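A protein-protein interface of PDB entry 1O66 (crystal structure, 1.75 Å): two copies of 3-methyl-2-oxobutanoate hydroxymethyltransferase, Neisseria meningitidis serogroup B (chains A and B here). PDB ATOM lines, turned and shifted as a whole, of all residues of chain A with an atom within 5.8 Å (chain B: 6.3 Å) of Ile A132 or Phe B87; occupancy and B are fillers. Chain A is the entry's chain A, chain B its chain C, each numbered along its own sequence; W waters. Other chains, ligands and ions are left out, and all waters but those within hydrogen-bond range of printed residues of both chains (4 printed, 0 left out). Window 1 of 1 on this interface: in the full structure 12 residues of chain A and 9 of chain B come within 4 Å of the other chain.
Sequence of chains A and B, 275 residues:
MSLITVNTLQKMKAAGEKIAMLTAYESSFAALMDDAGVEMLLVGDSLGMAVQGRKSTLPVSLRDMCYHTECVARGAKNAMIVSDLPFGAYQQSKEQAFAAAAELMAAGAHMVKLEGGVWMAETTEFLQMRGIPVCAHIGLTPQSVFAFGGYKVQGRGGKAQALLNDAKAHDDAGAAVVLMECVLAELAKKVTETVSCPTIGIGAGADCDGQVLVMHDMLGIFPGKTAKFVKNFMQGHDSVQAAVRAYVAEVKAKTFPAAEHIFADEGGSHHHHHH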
ATOM      1  N   PHE A  98     -31.133  -6.893 -13.016  1.00  0.00           N
ATOM      2  CA  PHE A  98     -30.061  -6.718 -13.980  1.00  0.00           C
ATOM      3  C   PHE A  98     -28.780  -6.301 -13.275  1.00  0.00           C
ATOM      4  O   PHE A  98     -27.700  -6.819 -13.567  1.00  0.00           O
ATOM      5  CB  PHE A  98     -30.418  -5.661 -15.022  1.00  0.00           C
ATOM      6  CG  PHE A  98     -29.281  -5.347 -15.952  1.00  0.00           C
ATOM      7  CD1 PHE A  98     -28.950  -6.217 -16.981  1.00  0.00           C
ATOM      8  CD2 PHE A  98     -28.493  -4.219 -15.743  1.00  0.00           C
ATOM      9  CE1 PHE A  98     -27.842  -5.976 -17.792  1.00  0.00           C
ATOM     10  CE2 PHE A  98     -27.387  -3.968 -16.545  1.00  0.00           C
ATOM     11  CZ  PHE A  98     -27.060  -4.848 -17.571  1.00  0.00           C
ATOM     12  N   ALA A 101     -27.394  -9.336 -11.438  1.00  0.00           N
ATOM     13  CA  ALA A 101     -26.884 -10.315 -12.385  1.00  0.00           C
ATOM     14  C   ALA A 101     -25.591  -9.823 -13.027  1.00  0.00           C
ATOM     15  O   ALA A 101     -24.674 -10.605 -13.291  1.00  0.00           O
ATOM     16  CB  ALA A 101     -27.937 -10.606 -13.450  1.00  0.00           C
ATOM     17  N   ALA A 102     -25.509  -8.518 -13.267  1.00  0.00           N
ATOM     18  CA  ALA A 102     -24.314  -7.942 -13.871  1.00  0.00           C
ATOM     19  C   ALA A 102     -23.107  -8.135 -12.952  1.00  0.00           C
ATOM     20  O   ALA A 102     -21.991  -8.370 -13.426  1.00  0.00           O
ATOM     21  CB  ALA A 102     -24.535  -6.463 -14.156  1.00  0.00           C
ATOM     22  N   MET A 105     -21.991 -11.731 -13.328  1.00  0.00           N
ATOM     23  CA  MET A 105     -21.281 -11.962 -14.583  1.00  0.00           C
ATOM     24  C   MET A 105     -19.865 -11.399 -14.427  1.00  0.00           C
ATOM     25  O   MET A 105     -18.885 -12.007 -14.858  1.00  0.00           O
ATOM     26  CB  MET A 105     -21.996 -11.271 -15.752  1.00  0.00           C
ATOM     27  CG  MET A 105     -23.420 -11.763 -16.040  1.00  0.00           C
ATOM     28  SD  MET A 105     -23.600 -13.659 -16.436  1.00  0.00           S
ATOM     29  CE  MET A 105     -22.792 -13.700 -18.199  1.00  0.00           C
ATOM     30  N   ALA A 106     -19.755 -10.229 -13.799  1.00  0.00           N
ATOM     31  CA  ALA A 106     -18.448  -9.613 -13.590  1.00  0.00           C
ATOM     32  C   ALA A 106     -17.567 -10.487 -12.696  1.00  0.00           C
ATOM     33  O   ALA A 106     -16.339 -10.441 -12.789  1.00  0.00           O
ATOM     34  CB  ALA A 106     -18.609  -8.227 -12.967  1.00  0.00           C
ATOM     35  N   MET A 111     -23.901 -17.494 -16.695  1.00  0.00           N
ATOM     36  CA  MET A 111     -25.356 -17.549 -16.700  1.00  0.00           C
ATOM     37  C   MET A 111     -25.777 -17.311 -15.259  1.00  0.00           C
ATOM     38  O   MET A 111     -24.996 -17.566 -14.342  1.00  0.00           O
ATOM     39  CB  MET A 111     -25.814 -18.946 -17.143  1.00  0.00           C
ATOM     40  CG  MET A 111     -27.314 -19.160 -17.217  1.00  0.00           C
ATOM     41  SD  MET A 111     -27.737 -21.009 -17.736  1.00  0.00           S
ATOM     42  CE  MET A 111     -27.125 -20.938 -19.563  1.00  0.00           C
ATOM     43  N   VAL A 112     -26.989 -16.804 -15.058  1.00  0.00           N
ATOM     44  CA  VAL A 112     -27.498 -16.586 -13.710  1.00  0.00           C
ATOM     45  C   VAL A 112     -28.805 -17.349 -13.563  1.00  0.00           C
ATOM     46  O   VAL A 112     -29.511 -17.578 -14.544  1.00  0.00           O
ATOM     47  CB  VAL A 112     -27.741 -15.087 -13.401  1.00  0.00           C
ATOM     48  CG1 VAL A 112     -26.438 -14.318 -13.551  1.00  0.00           C
ATOM     49  CG2 VAL A 112     -28.819 -14.523 -14.315  1.00  0.00           C
ATOM     50  N   THR A 124     -36.763 -12.173 -16.804  1.00  0.00           N
ATOM     51  CA  THR A 124     -35.969 -13.077 -17.626  1.00  0.00           C
ATOM     52  C   THR A 124     -35.716 -12.423 -18.979  1.00  0.00           C
ATOM     53  O   THR A 124     -34.596 -12.427 -19.485  1.00  0.00           O
ATOM     54  CB  THR A 124     -36.701 -14.413 -17.851  1.00  0.00           C
ATOM     55  OG1 THR A 124     -36.766 -15.124 -16.612  1.00  0.00           O
ATOM     56  CG2 THR A 124     -35.968 -15.267 -18.880  1.00  0.00           C
ATOM     57  N   LEU A 127     -33.141  -9.461 -18.846  1.00  0.00           N
ATOM     58  CA  LEU A 127     -31.759  -9.909 -18.728  1.00  0.00           C
ATOM     59  C   LEU A 127     -31.229 -10.560 -20.002  1.00  0.00           C
ATOM     60  O   LEU A 127     -30.137 -10.229 -20.464  1.00  0.00           O
ATOM     61  CB  LEU A 127     -31.629 -10.891 -17.557  1.00  0.00           C
ATOM     62  CG  LEU A 127     -31.234 -10.299 -16.199  1.00  0.00           C
ATOM     63  CD1 LEU A 127     -32.120  -9.114 -15.859  1.00  0.00           C
ATOM     64  CD2 LEU A 127     -31.327 -11.375 -15.126  1.00  0.00           C
ATOM     65  N   GLN A 128     -32.000 -11.482 -20.577  1.00  0.00           N
ATOM     66  CA  GLN A 128     -31.555 -12.176 -21.784  1.00  0.00           C
ATOM     67  C   GLN A 128     -31.277 -11.216 -22.938  1.00  0.00           C
ATOM     68  O   GLN A 128     -30.308 -11.386 -23.678  1.00  0.00           O
ATOM     69  CB  GLN A 128     -32.591 -13.222 -22.214  1.00  0.00           C
ATOM     70  CG  GLN A 128     -33.890 -12.631 -22.721  1.00  0.00           C
ATOM     71  CD  GLN A 128     -34.034 -12.742 -24.227  1.00  0.00           C
ATOM     72  OE1 GLN A 128     -33.045 -12.755 -24.958  1.00  0.00           O
ATOM     73  NE2 GLN A 128     -35.275 -12.808 -24.697  1.00  0.00           N
ATOM     74  N   MET A 129     -32.126 -10.206 -23.085  1.00  0.00           N
ATOM     75  CA  MET A 129     -31.959  -9.232 -24.156  1.00  0.00           C
ATOM     76  C   MET A 129     -30.670  -8.433 -23.989  1.00  0.00           C
ATOM     77  O   MET A 129     -30.115  -7.928 -24.962  1.00  0.00           O
ATOM     78  CB  MET A 129     -33.167  -8.288 -24.195  1.00  0.00           C
ATOM     79  CG  MET A 129     -34.421  -8.900 -24.777  1.00  0.00           C
ATOM     80  SD  MET A 129     -34.243  -9.162 -26.672  1.00  0.00           S
ATOM     81  CE  MET A 129     -34.639  -7.364 -27.249  1.00  0.00           C
ATOM     82  N   ARG A 130     -30.190  -8.338 -22.753  1.00  0.00           N
ATOM     83  CA  ARG A 130     -28.971  -7.597 -22.463  1.00  0.00           C
ATOM     84  C   ARG A 130     -27.715  -8.456 -22.376  1.00  0.00           C
ATOM     85  O   ARG A 130     -26.694  -8.031 -21.833  1.00  0.00           O
ATOM     86  CB  ARG A 130     -29.171  -6.776 -21.189  1.00  0.00           C
ATOM     87  CG  ARG A 130     -30.157  -5.654 -21.443  1.00  0.00           C
ATOM     88  CD  ARG A 130     -30.705  -4.991 -20.196  1.00  0.00           C
ATOM     89  NE  ARG A 130     -31.552  -3.872 -20.595  1.00  0.00           N
ATOM     90  CZ  ARG A 130     -32.691  -3.994 -21.274  1.00  0.00           C
ATOM     91  NH1 ARG A 130     -33.142  -5.194 -21.626  1.00  0.00           N
ATOM     92  NH2 ARG A 130     -33.366  -2.910 -21.638  1.00  0.00           N
ATOM     93  N   GLY A 131     -27.797  -9.667 -22.920  1.00  0.00           N
ATOM     94  CA  GLY A 131     -26.644 -10.547 -22.936  1.00  0.00           C
ATOM     95  C   GLY A 131     -26.414 -11.405 -21.711  1.00  0.00           C
ATOM     96  O   GLY A 131     -25.361 -12.027 -21.588  1.00  0.00           O
ATOM     97  N   ILE A 132     -27.375 -11.448 -20.798  1.00  0.00           N
ATOM     98  CA  ILE A 132     -27.216 -12.267 -19.606  1.00  0.00           C
ATOM     99  C   ILE A 132     -28.082 -13.520 -19.733  1.00  0.00           C
ATOM    100  O   ILE A 132     -29.308 -13.435 -19.687  1.00  0.00           O
ATOM    101  CB  ILE A 132     -27.621 -11.498 -18.327  1.00  0.00           C
ATOM    102  CG1 ILE A 132     -26.701 -10.291 -18.135  1.00  0.00           C
ATOM    103  CG2 ILE A 132     -27.519 -12.418 -17.106  1.00  0.00           C
ATOM    104  CD1 ILE A 132     -26.936  -9.521 -16.848  1.00  0.00           C
ATOM    105  N   PRO A 133     -27.454 -14.694 -19.920  1.00  0.00           N
ATOM    106  CA  PRO A 133     -28.226 -15.938 -20.046  1.00  0.00           C
ATOM    107  C   PRO A 133     -28.930 -16.205 -18.719  1.00  0.00           C
ATOM    108  O   PRO A 133     -28.352 -15.985 -17.655  1.00  0.00           O
ATOM    109  CB  PRO A 133     -27.152 -16.987 -20.344  1.00  0.00           C
ATOM    110  CG  PRO A 133     -26.066 -16.185 -21.022  1.00  0.00           C
ATOM    111  CD  PRO A 133     -26.022 -14.938 -20.176  1.00  0.00           C
ATOM    112  N   VAL A 134     -30.162 -16.693 -18.778  1.00  0.00           N
ATOM    113  CA  VAL A 134     -30.925 -16.945 -17.567  1.00  0.00           C
ATOM    114  C   VAL A 134     -31.415 -18.381 -17.417  1.00  0.00           C
ATOM    115  O   VAL A 134     -31.925 -18.973 -18.361  1.00  0.00           O
ATOM    116  CB  VAL A 134     -32.165 -16.016 -17.503  1.00  0.00           C
ATOM    117  CG1 VAL A 134     -33.052 -16.388 -16.310  1.00  0.00           C
ATOM    118  CG2 VAL A 134     -31.721 -14.563 -17.405  1.00  0.00           C
ATOM    119  N   ASP B  45     -13.788  -1.535 -24.401  1.00  0.00           N
ATOM    120  CA  ASP B  45     -13.801  -2.470 -23.287  1.00  0.00           C
ATOM    121  C   ASP B  45     -12.983  -3.713 -23.627  1.00  0.00           C
ATOM    122  O   ASP B  45     -12.852  -4.630 -22.822  1.00  0.00           O
ATOM    123  CB  ASP B  45     -15.238  -2.815 -22.859  1.00  0.00           C
ATOM    124  CG  ASP B  45     -16.008  -3.612 -23.895  1.00  0.00           C
ATOM    125  OD1 ASP B  45     -15.509  -3.819 -25.020  1.00  0.00           O
ATOM    126  OD2 ASP B  45     -17.139  -4.034 -23.560  1.00  0.00           O
ATOM    127  N   THR B  57     -14.969  -9.224 -21.796  1.00  0.00           N
ATOM    128  CA  THR B  57     -14.997  -7.802 -21.467  1.00  0.00           C
ATOM    129  C   THR B  57     -16.041  -7.456 -20.406  1.00  0.00           C
ATOM    130  O   THR B  57     -16.103  -6.318 -19.945  1.00  0.00           O
ATOM    131  CB  THR B  57     -15.320  -6.949 -22.710  1.00  0.00           C
ATOM    132  OG1 THR B  57     -16.665  -7.214 -23.126  1.00  0.00           O
ATOM    133  CG2 THR B  57     -14.372  -7.278 -23.858  1.00  0.00           C
ATOM    134  N   LEU B  58     -16.860  -8.425 -20.012  1.00  0.00           N
ATOM    135  CA  LEU B  58     -17.900  -8.140 -19.033  1.00  0.00           C
ATOM    136  C   LEU B  58     -17.438  -7.614 -17.669  1.00  0.00           C
ATOM    137  O   LEU B  58     -18.118  -6.782 -17.079  1.00  0.00           O
ATOM    138  CB  LEU B  58     -18.818  -9.358 -18.843  1.00  0.00           C
ATOM    139  CG  LEU B  58     -19.874  -9.559 -19.942  1.00  0.00           C
ATOM    140  CD1 LEU B  58     -19.198 -10.000 -21.235  1.00  0.00           C
ATOM    141  CD2 LEU B  58     -20.893 -10.600 -19.501  1.00  0.00           C
ATOM    142  N   PRO B  59     -16.285  -8.081 -17.150  1.00  0.00           N
ATOM    143  CA  PRO B  59     -15.837  -7.580 -15.842  1.00  0.00           C
ATOM    144  C   PRO B  59     -15.312  -6.140 -15.814  1.00  0.00           C
ATOM    145  O   PRO B  59     -15.074  -5.595 -14.736  1.00  0.00           O
ATOM    146  CB  PRO B  59     -14.749  -8.577 -15.435  1.00  0.00           C
ATOM    147  CG  PRO B  59     -15.131  -9.827 -16.173  1.00  0.00           C
ATOM    148  CD  PRO B  59     -15.529  -9.289 -17.523  1.00  0.00           C
ATOM    149  N   VAL B  60     -15.112  -5.530 -16.980  1.00  0.00           N
ATOM    150  CA  VAL B  60     -14.606  -4.155 -17.027  1.00  0.00           C
ATOM    151  C   VAL B  60     -15.611  -3.212 -16.371  1.00  0.00           C
ATOM    152  O   VAL B  60     -16.805  -3.311 -16.619  1.00  0.00           O
ATOM    153  CB  VAL B  60     -14.344  -3.711 -18.483  1.00  0.00           C
ATOM    154  CG1 VAL B  60     -13.861  -2.265 -18.514  1.00  0.00           C
ATOM    155  CG2 VAL B  60     -13.311  -4.639 -19.121  1.00  0.00           C
ATOM    156  N   SER B  61     -15.117  -2.295 -15.542  1.00  0.00           N
ATOM    157  CA  SER B  61     -15.978  -1.358 -14.824  1.00  0.00           C
ATOM    158  C   SER B  61     -15.943   0.042 -15.414  1.00  0.00           C
ATOM    159  O   SER B  61     -15.070   0.363 -16.217  1.00  0.00           O
ATOM    160  CB  SER B  61     -15.538  -1.258 -13.364  1.00  0.00           C
ATOM    161  OG  SER B  61     -14.246  -0.662 -13.265  1.00  0.00           O
ATOM    162  N   LEU B  85     -19.058   2.278 -23.198  1.00  0.00           N
ATOM    163  CA  LEU B  85     -19.824   2.237 -21.957  1.00  0.00           C
ATOM    164  C   LEU B  85     -19.638   0.755 -21.609  1.00  0.00           C
ATOM    165  O   LEU B  85     -19.976  -0.117 -22.411  1.00  0.00           O
ATOM    166  CB  LEU B  85     -21.300   2.542 -22.218  1.00  0.00           C
ATOM    167  CG  LEU B  85     -21.568   3.976 -22.677  1.00  0.00           C
ATOM    168  CD1 LEU B  85     -23.032   4.156 -23.036  1.00  0.00           C
ATOM    169  CD2 LEU B  85     -21.162   4.929 -21.567  1.00  0.00           C
ATOM    170  N   PRO B  86     -19.078   0.448 -20.429  1.00  0.00           N
ATOM    171  CA  PRO B  86     -18.863  -0.954 -20.052  1.00  0.00           C
ATOM    172  C   PRO B  86     -20.098  -1.741 -19.636  1.00  0.00           C
ATOM    173  O   PRO B  86     -21.091  -1.176 -19.193  1.00  0.00           O
ATOM    174  CB  PRO B  86     -17.833  -0.843 -18.937  1.00  0.00           C
ATOM    175  CG  PRO B  86     -18.276   0.384 -18.224  1.00  0.00           C
ATOM    176  CD  PRO B  86     -18.611   1.354 -19.364  1.00  0.00           C
ATOM    177  N   PHE B  87     -20.019  -3.059 -19.786  1.00  0.00           N
ATOM    178  CA  PHE B  87     -21.122  -3.944 -19.434  1.00  0.00           C
ATOM    179  C   PHE B  87     -21.615  -3.695 -18.014  1.00  0.00           C
ATOM    180  O   PHE B  87     -20.819  -3.643 -17.074  1.00  0.00           O
ATOM    181  CB  PHE B  87     -20.691  -5.406 -19.557  1.00  0.00           C
ATOM    182  CG  PHE B  87     -21.787  -6.383 -19.235  1.00  0.00           C
ATOM    183  CD1 PHE B  87     -22.747  -6.706 -20.189  1.00  0.00           C
ATOM    184  CD2 PHE B  87     -21.887  -6.940 -17.966  1.00  0.00           C
ATOM    185  CE1 PHE B  87     -23.798  -7.570 -19.881  1.00  0.00           C
ATOM    186  CE2 PHE B  87     -22.937  -7.807 -17.647  1.00  0.00           C
ATOM    187  CZ  PHE B  87     -23.892  -8.120 -18.609  1.00  0.00           C
ATOM    188  N   GLY B  88     -22.932  -3.548 -17.873  1.00  0.00           N
ATOM    189  CA  GLY B  88     -23.535  -3.324 -16.571  1.00  0.00           C
ATOM    190  C   GLY B  88     -23.698  -1.864 -16.182  1.00  0.00           C
ATOM    191  O   GLY B  88     -24.495  -1.527 -15.305  1.00  0.00           O
ATOM    192  N   ALA B  89     -22.956  -0.991 -16.850  1.00  0.00           N
ATOM    193  CA  ALA B  89     -22.995   0.430 -16.536  1.00  0.00           C
ATOM    194  C   ALA B  89     -24.032   1.257 -17.285  1.00  0.00           C
ATOM    195  O   ALA B  89     -24.260   2.414 -16.933  1.00  0.00           O
ATOM    196  CB  ALA B  89     -21.608   1.027 -16.760  1.00  0.00           C
ATOM    197  N   TYR B  90     -24.668   0.688 -18.304  1.00  0.00           N
ATOM    198  CA  TYR B  90     -25.628   1.472 -19.078  1.00  0.00           C
ATOM    199  C   TYR B  90     -26.929   0.815 -19.521  1.00  0.00           C
ATOM    200  O   TYR B  90     -27.838   1.503 -19.982  1.00  0.00           O
ATOM    201  CB  TYR B  90     -24.936   2.020 -20.329  1.00  0.00           C
ATOM    202  CG  TYR B  90     -24.569   0.949 -21.343  1.00  0.00           C
ATOM    203  CD1 TYR B  90     -23.511   0.065 -21.114  1.00  0.00           C
ATOM    204  CD2 TYR B  90     -25.287   0.816 -22.529  1.00  0.00           C
ATOM    205  CE1 TYR B  90     -23.176  -0.925 -22.053  1.00  0.00           C
ATOM    206  CE2 TYR B  90     -24.964  -0.165 -23.466  1.00  0.00           C
ATOM    207  CZ  TYR B  90     -23.911  -1.028 -23.224  1.00  0.00           C
ATOM    208  OH  TYR B  90     -23.597  -1.991 -24.158  1.00  0.00           O
ATOM    209  N   GLN B  91     -27.043  -0.500 -19.383  1.00  0.00           N
ATOM    210  CA  GLN B  91     -28.243  -1.174 -19.860  1.00  0.00           C
ATOM    211  C   GLN B  91     -29.453  -1.186 -18.934  1.00  0.00           C
ATOM    212  O   GLN B  91     -30.530  -1.632 -19.327  1.00  0.00           O
ATOM    213  CB  GLN B  91     -27.893  -2.608 -20.258  1.00  0.00           C
ATOM    214  CG  GLN B  91     -26.660  -2.709 -21.158  1.00  0.00           C
ATOM    215  CD  GLN B  91     -25.409  -3.128 -20.400  1.00  0.00           C
ATOM    216  OE1 GLN B  91     -25.037  -2.519 -19.402  1.00  0.00           O
ATOM    217  NE2 GLN B  91     -24.757  -4.181 -20.879  1.00  0.00           N
ATOM    218  N   GLN B 143     -20.149  -7.999 -25.721  1.00  0.00           N
ATOM    219  CA  GLN B 143     -20.793  -7.956 -24.415  1.00  0.00           C
ATOM    220  C   GLN B 143     -21.901  -9.000 -24.267  1.00  0.00           C
ATOM    221  O   GLN B 143     -22.359  -9.273 -23.156  1.00  0.00           O
ATOM    222  CB  GLN B 143     -21.348  -6.554 -24.147  1.00  0.00           C
ATOM    223  CG  GLN B 143     -20.295  -5.571 -23.670  1.00  0.00           C
ATOM    224  CD  GLN B 143     -20.833  -4.159 -23.540  1.00  0.00           C
ATOM    225  OE1 GLN B 143     -22.037  -3.956 -23.372  1.00  0.00           O
ATOM    226  NE2 GLN B 143     -19.939  -3.176 -23.598  1.00  0.00           N
ATOM    227  N   SER B 144     -22.317  -9.595 -25.382  1.00  0.00           N
ATOM    228  CA  SER B 144     -23.369 -10.609 -25.355  1.00  0.00           C
ATOM    229  C   SER B 144     -22.804 -11.980 -25.714  1.00  0.00           C
ATOM    230  O   SER B 144     -23.549 -12.897 -26.061  1.00  0.00           O
ATOM    231  CB  SER B 144     -24.482 -10.244 -26.342  1.00  0.00           C
ATOM    232  OG  SER B 144     -24.011 -10.282 -27.682  1.00  0.00           O
ATOM    233  N   PHE B 146     -21.759 -14.454 -23.992  1.00  0.00           N
ATOM    234  CA  PHE B 146     -22.263 -15.612 -23.260  1.00  0.00           C
ATOM    235  C   PHE B 146     -23.656 -16.047 -23.691  1.00  0.00           C
ATOM    236  O   PHE B 146     -24.065 -17.179 -23.430  1.00  0.00           O
ATOM    237  CB  PHE B 146     -22.228 -15.347 -21.753  1.00  0.00           C
ATOM    238  CG  PHE B 146     -20.835 -15.256 -21.197  1.00  0.00           C
ATOM    239  CD1 PHE B 146     -20.332 -14.047 -20.731  1.00  0.00           C
ATOM    240  CD2 PHE B 146     -20.012 -16.380 -21.171  1.00  0.00           C
ATOM    241  CE1 PHE B 146     -19.025 -13.954 -20.248  1.00  0.00           C
ATOM    242  CE2 PHE B 146     -18.706 -16.301 -20.691  1.00  0.00           C
ATOM    243  CZ  PHE B 146     -18.212 -15.082 -20.229  1.00  0.00           C
ATOM    244  N   ALA B 147     -24.377 -15.156 -24.360  1.00  0.00           N
ATOM    245  CA  ALA B 147     -25.720 -15.467 -24.836  1.00  0.00           C
ATOM    246  C   ALA B 147     -25.662 -15.943 -26.285  1.00  0.00           C
ATOM    247  O   ALA B 147     -26.079 -17.093 -26.541  1.00  0.00           O
ATOM    248  CB  ALA B 147     -26.614 -14.239 -24.723  1.00  0.00           C
HETATM  249  O   HOH W   1     -32.440  -0.234 -21.135  1.00  0.00           O
HETATM  250  O   HOH W   2     -22.674 -12.117 -22.500  1.00  0.00           O
HETATM  251  O   HOH W   3     -20.826  -5.899 -14.620  1.00  0.00           O
HETATM  252  O   HOH W   4     -26.012  -5.653 -22.895  1.00  0.00           O
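The backbone carbonyl oxygen (O) of Gln B91 lies within hydrogen-bond range of the guanidinium group (NE) of Arg A130, at 2.8 Å.
N of Ile A132 is in hydrogen-bond range of O of Leu A127 (3.0 Å).
N of Gly B88 sits at hydrogen-bond distance from OE1 of Gln B91 (2.8 Å).
The backbone NH (N) of Val A112 is in hydrogen-bond range of the backbone carbonyl oxygen (O) of Pro A133 (3.0 Å).
CE2 of Phe A98 touches CA of Gly B88, 3.9 Å away.
Gln B91 touches Phe A98.
Met A105 touches Leu B58 (CE to CD2, 3.9 Å).
CD1 of Phe B146 touches CE of Met A105 (3.5 Å).
CB of Pro B59 touches O of Ala A106 (3.6 Å).
Arg A130 touches Phe B87 (O to CE1, 3.5 Å).
CG1 of Ile A132 touches CZ of Phe B87, 3.6 Å away.
CG of Pro A133 touches O of Phe B146 (3.3 Å).
Pro A133 touches Ala B147.
Ile A132 touches just one residue of chain B: Phe B87.
Of chain A, only Arg A130 and Ile A132 come within 4 Å of Phe B87.
Of the printed residues of chain B, Phe A98 touches Gly B88 and Gln B91.
Of the printed residues of chain A, Ala B147 touches Pro A133 (3.9 Å).
Printed residues of chain A within 4 Å of Pro B59: Ala A106 (3.6 Å).
Thr B57 touches none of the printed residues of chain A.
The nearest residue of chain B that does not touch Ile A132 is Ala B147 (4.9 Å).
The nearest residue of chain A that does not touch Phe B87 is Ala A102 (4.02 Å).
Of the 16 printed residues of chain A, 6 touch a printed residue of chain B.
Hydrophobic or aromatic side chains of chain A within 4 Å of the printed part of chain B: Phe A98, Met A105, Ile A132 and Pro A133.
Of the 17 printed residues of chain B, 7 touch a printed residue of chain A.
Hydrophobic or aromatic side chains of chain B within 4 Å of the printed part of chain A: Leu B58, Pro B59, Phe B87 and Phe B146.
Among the printed residues, 10 pairs touch across the chains.
Among the printed residues, no Asp or Glu carboxylate lies within 4 Å of a Lys or Arg side-chain nitrogen of the other chain.
No position is printed for both chains.
Of the 10 pairs that touch across the chains among the printed residues, none has its exchanged pair printed and touching as well.
Water W4 lies within hydrogen-bond range of the backbone carbonyl oxygen (O) of Arg A130 (2.7 Å) and the side-chain amide nitrogen (NE2) of Gln B91 (2.8 Å).
Water W2 lies within hydrogen-bond range of the backbone carbonyl oxygen (O) of Gly A131 (2.8 Å), the backbone NH (N) of Phe B146 (2.9 Å) and the backbone carbonyl oxygen (O) of Gln B143 (2.9 Å).
Water W1 lies within hydrogen-bond range of the guanidinium group of Arg A130 (2.9 Å) and the backbone carbonyl oxygen of Gln B91 (3.0 Å).
Water W3 lies within hydrogen-bond range of the backbone carbonyl oxygen of Ala A102 (3.0 Å) and the backbone carbonyl oxygen of Phe B87 (3.3 Å).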
